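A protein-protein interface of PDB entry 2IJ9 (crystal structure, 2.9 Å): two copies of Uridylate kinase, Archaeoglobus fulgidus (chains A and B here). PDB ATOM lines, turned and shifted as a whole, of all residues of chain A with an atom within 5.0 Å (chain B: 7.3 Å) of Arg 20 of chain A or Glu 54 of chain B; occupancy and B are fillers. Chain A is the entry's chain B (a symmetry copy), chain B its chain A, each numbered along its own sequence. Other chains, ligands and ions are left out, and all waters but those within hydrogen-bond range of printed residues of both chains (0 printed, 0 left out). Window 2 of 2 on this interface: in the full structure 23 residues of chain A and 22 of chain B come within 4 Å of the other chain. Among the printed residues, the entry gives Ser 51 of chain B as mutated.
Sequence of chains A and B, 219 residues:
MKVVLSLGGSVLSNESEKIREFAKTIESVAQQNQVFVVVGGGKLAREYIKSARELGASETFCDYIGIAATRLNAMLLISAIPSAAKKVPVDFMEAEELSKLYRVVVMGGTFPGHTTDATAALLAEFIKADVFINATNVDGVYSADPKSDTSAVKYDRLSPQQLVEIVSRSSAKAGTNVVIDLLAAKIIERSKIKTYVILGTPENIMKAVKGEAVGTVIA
O of Glu 54 of chain B sits at hydrogen-bond distance from NH1 of Arg 20 of chain A, 3.1 Å away. The side-chain hydroxyl (OG) of Ser 16 of chain A lies close to the side-chain carboxylate (OE1) of Glu 54 of chain B.
NH2 of Arg 20 of chain A lies within hydrogen-bond range of OG of Ser 16 of chain A, at 3.2 Å.
Among the printed residues, pairs that only touch across the chains: Ser 16 of chain A with Leu 55 of chain B (3.5 Å), Ile 19 of chain A with Leu 55 of chain B (3.6 Å), Arg 20 of chain A with Leu 55 of chain B (3.9 Å) and Ala 80 of chain A with Leu 55 of chain B (3.7 Å).
Of the printed residues of chain B, Ser 16 of chain A touches Glu 54 and Leu 55. Of the printed residues of chain B, Ile 19 of chain A touches Leu 55. Of chain B, only Glu 54 and Leu 55 come within 4 Å of Arg 20 of chain A. Of the printed residues of chain B, Ala 80 of chain A touches Leu 55. Ile 49 of chain B touches none of the printed residues of chain A. Of chain A, only Ser 16 (3.1 Å) and Arg 20 (3.1 Å) come within 4 Å of Glu 54 of chain B. Of the printed residues of chain A, Leu 55 of chain B touches Ser 16 (3.5 Å), Ile 19 (3.6 Å), Arg 20 (3.9 Å) and Ala 80 (3.7 Å). The nearest printed residue of chain A that does not touch Glu 54 of chain B is Glu 17 of chain A (6.1 Å).
Of the 11 printed residues of chain A, 4 touch a printed residue of chain B. Hydrophobic or aromatic side chains of chain A within 4 Å of the printed part of chain B: Ile 19 and Ala 80. Printed residues of chain B that touch a printed residue of chain A: Glu 54 and Leu 55. Among the printed residues, no Asp or Glu carboxylate lies within 4 Å of a Lys or Arg side-chain nitrogen of the other chain.
No position is printed for both chains.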
ATOM      1  N   GLU A  15      21.272  24.536 -14.085  1.00  0.00           N
ATOM      2  CA  GLU A  15      21.887  25.862 -14.183  1.00  0.00           C
ATOM      3  C   GLU A  15      23.410  25.692 -14.145  1.00  0.00           C
ATOM      4  O   GLU A  15      23.974  25.286 -13.117  1.00  0.00           O
ATOM      5  CB  GLU A  15      21.432  26.772 -13.033  1.00  0.00           C
ATOM      6  CG  GLU A  15      20.120  26.366 -12.362  1.00  0.00           C
ATOM      7  CD  GLU A  15      20.279  25.316 -11.254  1.00  0.00           C
ATOM      8  OE1 GLU A  15      21.400  24.802 -11.039  1.00  0.00           O
ATOM      9  OE2 GLU A  15      19.264  25.004 -10.596  1.00  0.00           O
ATOM     10  N   SER A  16      24.063  26.002 -15.262  1.00  0.00           N
ATOM     11  CA  SER A  16      25.509  25.778 -15.441  1.00  0.00           C
ATOM     12  C   SER A  16      26.410  26.224 -14.284  1.00  0.00           C
ATOM     13  O   SER A  16      27.222  25.447 -13.789  1.00  0.00           O
ATOM     14  CB  SER A  16      25.982  26.445 -16.727  1.00  0.00           C
ATOM     15  OG  SER A  16      27.326  26.105 -17.016  1.00  0.00           O
ATOM     16  N   GLU A  17      26.258  27.476 -13.861  1.00  0.00           N
ATOM     17  CA  GLU A  17      27.065  28.032 -12.781  1.00  0.00           C
ATOM     18  C   GLU A  17      26.781  27.393 -11.412  1.00  0.00           C
ATOM     19  O   GLU A  17      27.723  27.129 -10.658  1.00  0.00           O
ATOM     20  CB  GLU A  17      26.946  29.569 -12.726  1.00  0.00           C
ATOM     21  CG  GLU A  17      25.599  30.140 -12.213  1.00  0.00           C
ATOM     22  CD  GLU A  17      24.438  29.961 -13.193  1.00  0.00           C
ATOM     23  OE1 GLU A  17      24.658  30.107 -14.417  1.00  0.00           O
ATOM     24  OE2 GLU A  17      23.305  29.678 -12.734  1.00  0.00           O
ATOM     25  N   LYS A  18      25.507  27.133 -11.097  1.00  0.00           N
ATOM     26  CA  LYS A  18      25.155  26.588  -9.784  1.00  0.00           C
ATOM     27  C   LYS A  18      25.710  25.181  -9.666  1.00  0.00           C
ATOM     28  O   LYS A  18      26.218  24.779  -8.615  1.00  0.00           O
ATOM     29  CB  LYS A  18      23.644  26.586  -9.545  1.00  0.00           C
ATOM     30  CG  LYS A  18      23.280  26.460  -8.071  1.00  0.00           C
ATOM     31  CD  LYS A  18      21.808  26.146  -7.826  1.00  0.00           C
ATOM     32  CE  LYS A  18      21.452  26.429  -6.359  1.00  0.00           C
ATOM     33  NZ  LYS A  18      20.152  25.847  -5.911  1.00  0.00           N
ATOM     34  N   ILE A  19      25.624  24.445 -10.769  1.00  0.00           N
ATOM     35  CA  ILE A  19      26.197  23.105 -10.857  1.00  0.00           C
ATOM     36  C   ILE A  19      27.725  23.163 -10.685  1.00  0.00           C
ATOM     37  O   ILE A  19      28.316  22.396  -9.906  1.00  0.00           O
ATOM     38  CB  ILE A  19      25.759  22.389 -12.168  1.00  0.00           C
ATOM     39  CG1 ILE A  19      24.279  21.984 -12.058  1.00  0.00           C
ATOM     40  CG2 ILE A  19      26.657  21.178 -12.475  1.00  0.00           C
ATOM     41  CD1 ILE A  19      23.685  21.293 -13.296  1.00  0.00           C
ATOM     42  N   ARG A  20      28.357  24.107 -11.373  1.00  0.00           N
ATOM     43  CA  ARG A  20      29.782  24.304 -11.174  1.00  0.00           C
ATOM     44  C   ARG A  20      30.066  24.551  -9.685  1.00  0.00           C
ATOM     45  O   ARG A  20      31.022  24.011  -9.146  1.00  0.00           O
ATOM     46  CB  ARG A  20      30.317  25.433 -12.057  1.00  0.00           C
ATOM     47  CG  ARG A  20      31.788  25.274 -12.424  1.00  0.00           C
ATOM     48  CD  ARG A  20      32.319  26.458 -13.222  1.00  0.00           C
ATOM     49  NE  ARG A  20      31.341  26.939 -14.197  1.00  0.00           N
ATOM     50  CZ  ARG A  20      31.246  26.504 -15.450  1.00  0.00           C
ATOM     51  NH1 ARG A  20      32.077  25.569 -15.901  1.00  0.00           N
ATOM     52  NH2 ARG A  20      30.317  27.010 -16.254  1.00  0.00           N
ATOM     53  N   GLU A  21      29.194  25.312  -9.023  1.00  0.00           N
ATOM     54  CA  GLU A  21      29.345  25.639  -7.612  1.00  0.00           C
ATOM     55  C   GLU A  21      29.248  24.390  -6.736  1.00  0.00           C
ATOM     56  O   GLU A  21      30.074  24.200  -5.836  1.00  0.00           O
ATOM     57  CB  GLU A  21      28.298  26.681  -7.195  1.00  0.00           C
ATOM     58  CG  GLU A  21      28.664  27.524  -5.974  1.00  0.00           C
ATOM     59  CD  GLU A  21      27.504  28.381  -5.461  1.00  0.00           C
ATOM     60  OE1 GLU A  21      26.333  27.969  -5.625  1.00  0.00           O
ATOM     61  OE2 GLU A  21      27.763  29.462  -4.882  1.00  0.00           O
ATOM     62  N   PHE A  22      28.262  23.534  -7.006  1.00  0.00           N
ATOM     63  CA  PHE A  22      28.123  22.262  -6.275  1.00  0.00           C
ATOM     64  C   PHE A  22      29.279  21.284  -6.510  1.00  0.00           C
ATOM     65  O   PHE A  22      29.828  20.721  -5.552  1.00  0.00           O
ATOM     66  CB  PHE A  22      26.804  21.573  -6.616  1.00  0.00           C
ATOM     67  CG  PHE A  22      25.627  22.115  -5.868  1.00  0.00           C
ATOM     68  CD1 PHE A  22      25.361  21.709  -4.564  1.00  0.00           C
ATOM     69  CD2 PHE A  22      24.774  23.027  -6.468  1.00  0.00           C
ATOM     70  CE1 PHE A  22      24.263  22.211  -3.874  1.00  0.00           C
ATOM     71  CE2 PHE A  22      23.680  23.532  -5.787  1.00  0.00           C
ATOM     72  CZ  PHE A  22      23.423  23.123  -4.489  1.00  0.00           C
ATOM     73  N   ALA A  23      29.640  21.085  -7.779  1.00  0.00           N
ATOM     74  CA  ALA A  23      30.760  20.217  -8.139  1.00  0.00           C
ATOM     75  C   ALA A  23      32.024  20.626  -7.397  1.00  0.00           C
ATOM     76  O   ALA A  23      32.664  19.803  -6.746  1.00  0.00           O
ATOM     77  CB  ALA A  23      31.004  20.231  -9.638  1.00  0.00           C
ATOM     78  N   LYS A  24      32.353  21.912  -7.467  1.00  0.00           N
ATOM     79  CA  LYS A  24      33.555  22.433  -6.830  1.00  0.00           C
ATOM     80  C   LYS A  24      33.624  22.096  -5.346  1.00  0.00           C
ATOM     81  O   LYS A  24      34.691  21.716  -4.843  1.00  0.00           O
ATOM     82  CB  LYS A  24      33.697  23.936  -7.069  1.00  0.00           C
ATOM     83  CG  LYS A  24      34.237  24.273  -8.462  1.00  0.00           C
ATOM     84  CD  LYS A  24      34.971  25.599  -8.483  1.00  0.00           C
ATOM     85  CE  LYS A  24      35.592  25.856  -9.847  1.00  0.00           C
ATOM     86  NZ  LYS A  24      36.425  27.091  -9.857  1.00  0.00           N
ATOM     87  N   ALA A  80      30.727  17.982 -14.590  1.00  0.00           N
ATOM     88  CA  ALA A  80      31.270  19.044 -13.773  1.00  0.00           C
ATOM     89  C   ALA A  80      32.374  18.615 -12.812  1.00  0.00           C
ATOM     90  O   ALA A  80      33.283  19.391 -12.549  1.00  0.00           O
ATOM     91  CB  ALA A  80      30.152  19.756 -13.033  1.00  0.00           C
ATOM     92  N   GLU B  47      19.931  20.722 -24.824  1.00  0.00           N
ATOM     93  CA  GLU B  47      20.033  21.395 -23.543  1.00  0.00           C
ATOM     94  C   GLU B  47      21.143  20.760 -22.738  1.00  0.00           C
ATOM     95  O   GLU B  47      22.059  21.446 -22.275  1.00  0.00           O
ATOM     96  CB  GLU B  47      18.690  21.240 -22.820  1.00  0.00           C
ATOM     97  CG  GLU B  47      18.368  22.205 -21.679  1.00  0.00           C
ATOM     98  CD  GLU B  47      16.933  22.007 -21.165  1.00  0.00           C
ATOM     99  OE1 GLU B  47      16.700  22.190 -19.948  1.00  0.00           O
ATOM    100  OE2 GLU B  47      16.037  21.656 -21.976  1.00  0.00           O
ATOM    101  N   TYR B  48      21.077  19.441 -22.592  1.00  0.00           N
ATOM    102  CA  TYR B  48      21.960  18.768 -21.664  1.00  0.00           C
ATOM    103  C   TYR B  48      23.400  18.699 -22.143  1.00  0.00           C
ATOM    104  O   TYR B  48      24.331  18.790 -21.344  1.00  0.00           O
ATOM    105  CB  TYR B  48      21.415  17.401 -21.283  1.00  0.00           C
ATOM    106  CG  TYR B  48      20.508  17.457 -20.080  1.00  0.00           C
ATOM    107  CD1 TYR B  48      19.180  17.845 -20.209  1.00  0.00           C
ATOM    108  CD2 TYR B  48      20.983  17.135 -18.806  1.00  0.00           C
ATOM    109  CE1 TYR B  48      18.342  17.887 -19.110  1.00  0.00           C
ATOM    110  CE2 TYR B  48      20.148  17.181 -17.705  1.00  0.00           C
ATOM    111  CZ  TYR B  48      18.835  17.560 -17.868  1.00  0.00           C
ATOM    112  OH  TYR B  48      18.004  17.608 -16.790  1.00  0.00           O
ATOM    113  N   ILE B  49      23.571  18.534 -23.449  1.00  0.00           N
ATOM    114  CA  ILE B  49      24.897  18.522 -24.050  1.00  0.00           C
ATOM    115  C   ILE B  49      25.502  19.906 -23.872  1.00  0.00           C
ATOM    116  O   ILE B  49      26.629  20.039 -23.382  1.00  0.00           O
ATOM    117  CB  ILE B  49      24.843  18.173 -25.534  1.00  0.00           C
ATOM    118  CG1 ILE B  49      24.367  16.740 -25.717  1.00  0.00           C
ATOM    119  CG2 ILE B  49      26.217  18.288 -26.136  1.00  0.00           C
ATOM    120  CD1 ILE B  49      23.817  16.469 -27.081  1.00  0.00           C
ATOM    121  N   LYS B  50      24.731  20.927 -24.250  1.00  0.00           N
ATOM    122  CA  LYS B  50      25.088  22.318 -23.998  1.00  0.00           C
ATOM    123  C   LYS B  50      25.636  22.455 -22.570  1.00  0.00           C
ATOM    124  O   LYS B  50      26.813  22.795 -22.384  1.00  0.00           O
ATOM    125  CB  LYS B  50      23.863  23.218 -24.214  1.00  0.00           C
ATOM    126  CG  LYS B  50      24.129  24.707 -24.483  1.00  0.00           C
ATOM    127  CD  LYS B  50      22.869  25.547 -24.183  1.00  0.00           C
ATOM    128  CE  LYS B  50      23.100  27.037 -24.354  1.00  0.00           C
ATOM    129  NZ  LYS B  50      22.037  27.844 -23.687  1.00  0.00           N
ATOM    130  N   SER B  51      24.804  22.138 -21.574  1.00  0.00           N
ATOM    131  CA  SER B  51      25.208  22.239 -20.171  1.00  0.00           C
ATOM    132  C   SER B  51      26.429  21.370 -19.858  1.00  0.00           C
ATOM    133  O   SER B  51      27.297  21.760 -19.083  1.00  0.00           O
ATOM    134  CB  SER B  51      24.044  21.874 -19.245  1.00  0.00           C
ATOM    135  OG  SER B  51      23.218  22.991 -18.949  1.00  0.00           O
ATOM    136  N   ALA B  52      26.494  20.192 -20.474  1.00  0.00           N
ATOM    137  CA  ALA B  52      27.568  19.248 -20.177  1.00  0.00           C
ATOM    138  C   ALA B  52      28.894  19.711 -20.763  1.00  0.00           C
ATOM    139  O   ALA B  52      29.929  19.577 -20.112  1.00  0.00           O
ATOM    140  CB  ALA B  52      27.217  17.851 -20.667  1.00  0.00           C
ATOM    141  N   ARG B  53      28.851  20.254 -21.981  1.00  0.00           N
ATOM    142  CA  ARG B  53      30.008  20.926 -22.581  1.00  0.00           C
ATOM    143  C   ARG B  53      30.458  22.104 -21.719  1.00  0.00           C
ATOM    144  O   ARG B  53      31.648  22.227 -21.391  1.00  0.00           O
ATOM    145  CB  ARG B  53      29.673  21.440 -23.972  1.00  0.00           C
ATOM    146  CG  ARG B  53      30.021  20.506 -25.103  1.00  0.00           C
ATOM    147  CD  ARG B  53      29.463  21.068 -26.397  1.00  0.00           C
ATOM    148  NE  ARG B  53      29.273  20.045 -27.419  1.00  0.00           N
ATOM    149  CZ  ARG B  53      28.397  20.139 -28.415  1.00  0.00           C
ATOM    150  NH1 ARG B  53      27.613  21.205 -28.524  1.00  0.00           N
ATOM    151  NH2 ARG B  53      28.296  19.157 -29.301  1.00  0.00           N
ATOM    152  N   GLU B  54      29.496  22.953 -21.349  1.00  0.00           N
ATOM    153  CA  GLU B  54      29.739  24.083 -20.464  1.00  0.00           C
ATOM    154  C   GLU B  54      30.511  23.676 -19.211  1.00  0.00           C
ATOM    155  O   GLU B  54      31.329  24.442 -18.707  1.00  0.00           O
ATOM    156  CB  GLU B  54      28.412  24.755 -20.084  1.00  0.00           C
ATOM    157  CG  GLU B  54      27.897  25.768 -21.116  1.00  0.00           C
ATOM    158  CD  GLU B  54      26.411  26.088 -20.962  1.00  0.00           C
ATOM    159  OE1 GLU B  54      25.899  26.135 -19.820  1.00  0.00           O
ATOM    160  OE2 GLU B  54      25.748  26.297 -21.997  1.00  0.00           O
ATOM    161  N   LEU B  55      30.263  22.463 -18.723  1.00  0.00           N
ATOM    162  CA  LEU B  55      30.903  21.989 -17.505  1.00  0.00           C
ATOM    163  C   LEU B  55      32.204  21.240 -17.786  1.00  0.00           C
ATOM    164  O   LEU B  55      32.874  20.779 -16.863  1.00  0.00           O
ATOM    165  CB  LEU B  55      29.930  21.144 -16.694  1.00  0.00           C
ATOM    166  CG  LEU B  55      28.711  21.923 -16.194  1.00  0.00           C
ATOM    167  CD1 LEU B  55      27.530  20.978 -15.946  1.00  0.00           C
ATOM    168  CD2 LEU B  55      29.034  22.748 -14.951  1.00  0.00           C
ATOM    169  N   GLY B  56      32.560  21.131 -19.065  1.00  0.00           N
ATOM    170  CA  GLY B  56      33.844  20.551 -19.477  1.00  0.00           C
ATOM    171  C   GLY B  56      33.854  19.045 -19.673  1.00  0.00           C
ATOM    172  O   GLY B  56      34.788  18.367 -19.249  1.00  0.00           O
ATOM    173  N   ALA B  57      32.810  18.532 -20.319  1.00  0.00           N
ATOM    174  CA  ALA B  57      32.704  17.117 -20.658  1.00  0.00           C
ATOM    175  C   ALA B  57      33.545  16.802 -21.868  1.00  0.00           C
ATOM    176  O   ALA B  57      33.712  17.634 -22.762  1.00  0.00           O
ATOM    177  CB  ALA B  57      31.262  16.749 -20.958  1.00  0.00           C
ATOM    178  N   CYS B  62      29.641  13.496 -23.662  1.00  0.00           N
ATOM    179  CA  CYS B  62      28.529  14.232 -24.245  1.00  0.00           C
ATOM    180  C   CYS B  62      27.695  13.262 -25.043  1.00  0.00           C
ATOM    181  O   CYS B  62      26.465  13.209 -24.888  1.00  0.00           O
ATOM    182  CB  CYS B  62      29.015  15.359 -25.162  1.00  0.00           C
ATOM    183  SG  CYS B  62      29.457  16.858 -24.294  1.00  0.00           S
